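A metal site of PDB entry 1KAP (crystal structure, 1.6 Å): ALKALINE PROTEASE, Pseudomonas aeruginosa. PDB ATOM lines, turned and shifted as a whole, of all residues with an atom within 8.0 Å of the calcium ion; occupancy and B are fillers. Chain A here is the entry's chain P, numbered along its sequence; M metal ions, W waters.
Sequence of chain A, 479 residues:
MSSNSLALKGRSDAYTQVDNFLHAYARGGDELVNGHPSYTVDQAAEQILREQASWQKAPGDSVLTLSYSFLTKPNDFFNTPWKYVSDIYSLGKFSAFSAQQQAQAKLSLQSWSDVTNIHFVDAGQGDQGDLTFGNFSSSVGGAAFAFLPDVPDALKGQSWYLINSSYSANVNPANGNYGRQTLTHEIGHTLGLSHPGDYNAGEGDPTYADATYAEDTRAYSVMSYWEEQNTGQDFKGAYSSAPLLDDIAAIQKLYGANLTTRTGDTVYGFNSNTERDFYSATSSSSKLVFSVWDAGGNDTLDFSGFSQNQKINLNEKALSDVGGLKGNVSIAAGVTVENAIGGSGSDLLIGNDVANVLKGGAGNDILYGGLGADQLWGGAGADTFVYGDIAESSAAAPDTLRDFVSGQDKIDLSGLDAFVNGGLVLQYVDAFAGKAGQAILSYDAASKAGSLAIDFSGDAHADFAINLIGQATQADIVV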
ATOM      1  N   PHE A 432      18.163  14.461   5.307  1.00  0.00           N
ATOM      2  CA  PHE A 432      17.116  14.467   6.330  1.00  0.00           C
ATOM      3  C   PHE A 432      16.606  13.046   6.519  1.00  0.00           C
ATOM      4  O   PHE A 432      16.458  12.319   5.540  1.00  0.00           O
ATOM      5  CB  PHE A 432      15.954  15.365   5.922  1.00  0.00           C
ATOM      6  CG  PHE A 432      16.304  16.838   5.869  1.00  0.00           C
ATOM      7  CD1 PHE A 432      16.988  17.446   6.919  1.00  0.00           C
ATOM      8  CD2 PHE A 432      15.954  17.618   4.773  1.00  0.00           C
ATOM      9  CE1 PHE A 432      17.299  18.805   6.877  1.00  0.00           C
ATOM     10  CE2 PHE A 432      16.266  18.970   4.718  1.00  0.00           C
ATOM     11  CZ  PHE A 432      16.945  19.561   5.784  1.00  0.00           C
ATOM     12  N   LYS A 435      13.577  13.864  11.379  1.00  0.00           N
ATOM     13  CA  LYS A 435      13.810  14.278  12.759  1.00  0.00           C
ATOM     14  C   LYS A 435      13.903  15.812  12.822  1.00  0.00           C
ATOM     15  O   LYS A 435      14.623  16.430  12.037  1.00  0.00           O
ATOM     16  CB  LYS A 435      15.093  13.645  13.297  1.00  0.00           C
ATOM     17  CG  LYS A 435      15.328  13.909  14.769  1.00  0.00           C
ATOM     18  CD  LYS A 435      16.705  13.418  15.226  1.00  0.00           C
ATOM     19  CE  LYS A 435      16.981  13.895  16.652  1.00  0.00           C
ATOM     20  NZ  LYS A 435      18.367  13.551  17.131  1.00  0.00           N
ATOM     21  N   ALA A 436      13.149  16.416  13.744  1.00  0.00           N
ATOM     22  CA  ALA A 436      13.123  17.862  13.907  1.00  0.00           C
ATOM     23  C   ALA A 436      14.476  18.447  14.320  1.00  0.00           C
ATOM     24  O   ALA A 436      15.163  17.899  15.171  1.00  0.00           O
ATOM     25  CB  ALA A 436      12.059  18.248  14.919  1.00  0.00           C
ATOM     26  N   GLY A 437      14.856  19.555  13.704  1.00  0.00           N
ATOM     27  CA  GLY A 437      16.113  20.180  14.045  1.00  0.00           C
ATOM     28  C   GLY A 437      17.302  19.764  13.200  1.00  0.00           C
ATOM     29  O   GLY A 437      18.427  20.201  13.465  1.00  0.00           O
ATOM     30  N   ILE A 454      17.031  23.779   6.880  1.00  0.00           N
ATOM     31  CA  ILE A 454      16.696  23.174   8.167  1.00  0.00           C
ATOM     32  C   ILE A 454      15.292  22.595   8.190  1.00  0.00           C
ATOM     33  O   ILE A 454      14.339  23.207   7.708  1.00  0.00           O
ATOM     34  CB  ILE A 454      16.824  24.189   9.349  1.00  0.00           C
ATOM     35  CG1 ILE A 454      18.192  24.889   9.324  1.00  0.00           C
ATOM     36  CG2 ILE A 454      16.619  23.462  10.692  1.00  0.00           C
ATOM     37  CD1 ILE A 454      18.411  25.878  10.469  1.00  0.00           C
ATOM     38  N   ASP A 455      15.185  21.371   8.703  1.00  0.00           N
ATOM     39  CA  ASP A 455      13.910  20.710   8.857  1.00  0.00           C
ATOM     40  C   ASP A 455      13.504  20.889  10.322  1.00  0.00           C
ATOM     41  O   ASP A 455      13.979  20.178  11.217  1.00  0.00           O
ATOM     42  CB  ASP A 455      14.010  19.223   8.487  1.00  0.00           C
ATOM     43  CG  ASP A 455      12.696  18.483   8.683  1.00  0.00           C
ATOM     44  OD1 ASP A 455      11.630  19.135   8.748  1.00  0.00           O
ATOM     45  OD2 ASP A 455      12.733  17.253   8.773  1.00  0.00           O
ATOM     46  N   PHE A 456      12.691  21.891  10.573  1.00  0.00           N
ATOM     47  CA  PHE A 456      12.215  22.163  11.925  1.00  0.00           C
ATOM     48  C   PHE A 456      11.065  21.260  12.330  1.00  0.00           C
ATOM     49  O   PHE A 456      10.894  20.985  13.522  1.00  0.00           O
ATOM     50  CB  PHE A 456      11.767  23.625  12.028  1.00  0.00           C
ATOM     51  CG  PHE A 456      12.899  24.602  12.150  1.00  0.00           C
ATOM     52  CD1 PHE A 456      13.500  24.820  13.384  1.00  0.00           C
ATOM     53  CD2 PHE A 456      13.340  25.310  11.041  1.00  0.00           C
ATOM     54  CE1 PHE A 456      14.556  25.738  13.517  1.00  0.00           C
ATOM     55  CE2 PHE A 456      14.397  26.224  11.152  1.00  0.00           C
ATOM     56  CZ  PHE A 456      14.999  26.440  12.396  1.00  0.00           C
ATOM     57  N   SER A 457      10.288  20.794  11.363  1.00  0.00           N
ATOM     58  CA  SER A 457       9.119  19.953  11.662  1.00  0.00           C
ATOM     59  C   SER A 457       9.389  18.466  11.810  1.00  0.00           C
ATOM     60  O   SER A 457       8.611  17.756  12.457  1.00  0.00           O
ATOM     61  CB  SER A 457       8.024  20.180  10.628  1.00  0.00           C
ATOM     62  OG  SER A 457       8.493  19.901   9.327  1.00  0.00           O
ATOM     63  N   GLY A 458      10.456  17.973  11.195  1.00  0.00           N
ATOM     64  CA  GLY A 458      10.784  16.571  11.300  1.00  0.00           C
ATOM     65  C   GLY A 458      10.134  15.670  10.274  1.00  0.00           C
ATOM     66  O   GLY A 458      10.041  14.460  10.487  1.00  0.00           O
ATOM     67  N   ASP A 459       9.690  16.234   9.154  1.00  0.00           N
ATOM     68  CA  ASP A 459       9.059  15.443   8.107  1.00  0.00           C
ATOM     69  C   ASP A 459      10.023  15.219   6.943  1.00  0.00           C
ATOM     70  O   ASP A 459       9.612  14.851   5.834  1.00  0.00           O
ATOM     71  CB  ASP A 459       7.767  16.144   7.622  1.00  0.00           C
ATOM     72  CG  ASP A 459       8.038  17.445   6.885  1.00  0.00           C
ATOM     73  OD1 ASP A 459       9.139  18.030   7.040  1.00  0.00           O
ATOM     74  OD2 ASP A 459       7.141  17.890   6.128  1.00  0.00           O
ATOM     75  N   ALA A 460      11.304  15.477   7.192  1.00  0.00           N
ATOM     76  CA  ALA A 460      12.352  15.324   6.188  1.00  0.00           C
ATOM     77  C   ALA A 460      12.210  16.315   5.031  1.00  0.00           C
ATOM     78  O   ALA A 460      12.693  16.064   3.925  1.00  0.00           O
ATOM     79  CB  ALA A 460      12.429  13.873   5.653  1.00  0.00           C
ATOM     80  N   HIS A 461      11.501  17.427   5.273  1.00  0.00           N
ATOM     81  CA  HIS A 461      11.341  18.485   4.263  1.00  0.00           C
ATOM     82  C   HIS A 461      11.801  19.776   4.931  1.00  0.00           C
ATOM     83  O   HIS A 461      11.410  20.071   6.052  1.00  0.00           O
ATOM     84  CB  HIS A 461       9.883  18.650   3.832  1.00  0.00           C
ATOM     85  CG  HIS A 461       9.365  17.514   3.007  1.00  0.00           C
ATOM     86  ND1 HIS A 461       9.935  17.142   1.814  1.00  0.00           N
ATOM     87  CD2 HIS A 461       8.338  16.651   3.234  1.00  0.00           C
ATOM     88  CE1 HIS A 461       9.293  16.085   1.339  1.00  0.00           C
ATOM     89  NE2 HIS A 461       8.327  15.771   2.175  1.00  0.00           N
ATOM     90  N   ALA A 462      12.691  20.495   4.255  1.00  0.00           N
ATOM     91  CA  ALA A 462      13.199  21.761   4.774  1.00  0.00           C
ATOM     92  C   ALA A 462      12.074  22.795   4.917  1.00  0.00           C
ATOM     93  O   ALA A 462      11.248  22.962   4.007  1.00  0.00           O
ATOM     94  CB  ALA A 462      14.295  22.302   3.857  1.00  0.00           C
ATOM     95  N   ASP A 463      12.038  23.445   6.069  1.00  0.00           N
ATOM     96  CA  ASP A 463      11.050  24.480   6.367  1.00  0.00           C
ATOM     97  C   ASP A 463      11.673  25.869   6.210  1.00  0.00           C
ATOM     98  O   ASP A 463      11.001  26.842   5.873  1.00  0.00           O
ATOM     99  CB  ASP A 463      10.579  24.342   7.806  1.00  0.00           C
ATOM    100  CG  ASP A 463      10.034  22.972   8.108  1.00  0.00           C
ATOM    101  OD1 ASP A 463       8.969  22.647   7.556  1.00  0.00           O
ATOM    102  OD2 ASP A 463      10.659  22.244   8.890  1.00  0.00           O
ATOM    103  N   PHE A 464      12.991  25.929   6.396  1.00  0.00           N
ATOM    104  CA  PHE A 464      13.756  27.161   6.378  1.00  0.00           C
ATOM    105  C   PHE A 464      15.009  26.916   5.536  1.00  0.00           C
ATOM    106  O   PHE A 464      15.633  25.854   5.632  1.00  0.00           O
ATOM    107  CB  PHE A 464      14.123  27.470   7.830  1.00  0.00           C
ATOM    108  CG  PHE A 464      14.951  28.705   8.026  1.00  0.00           C
ATOM    109  CD1 PHE A 464      14.347  29.954   8.174  1.00  0.00           C
ATOM    110  CD2 PHE A 464      16.345  28.611   8.149  1.00  0.00           C
ATOM    111  CE1 PHE A 464      15.120  31.095   8.442  1.00  0.00           C
ATOM    112  CE2 PHE A 464      17.129  29.745   8.414  1.00  0.00           C
ATOM    113  CZ  PHE A 464      16.506  30.989   8.563  1.00  0.00           C
HETATM  114 CA    CA M   1       9.844  20.156   7.640  1.00  0.00          CA
HETATM  115  O   HOH W   1       7.974  20.695   5.599  1.00  0.00           O
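The side-chain carboxylate of Asp 455 lies close to the backbone NH of Gly 458, at 3.4 Å.
N of Ala 460 is in hydrogen-bond range of OD2 of Asp 455.
O of Asp 455 sits at hydrogen-bond distance from N of Gly 437, at 2.7 Å.
OD2 of Asp 463 sits close to N of Phe 456, 2.7 Å away.
O of Ile 454 is in hydrogen-bond range of N of Asp 463.
Of the 15 residues printed, 5 come within 4 Å of the calcium ion.
The nearest printed residue that does not touch the calcium ion is Gly 458 (4.2 Å).
The calcium ion is bound by OG of Ser 457, O of His 461, OD1 of Asp 459, OD1 of Asp 455, OD2 of Asp 463, OD1 of Asp 463 and water W1.
The calcium ion has seven donor atoms within binding distance.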
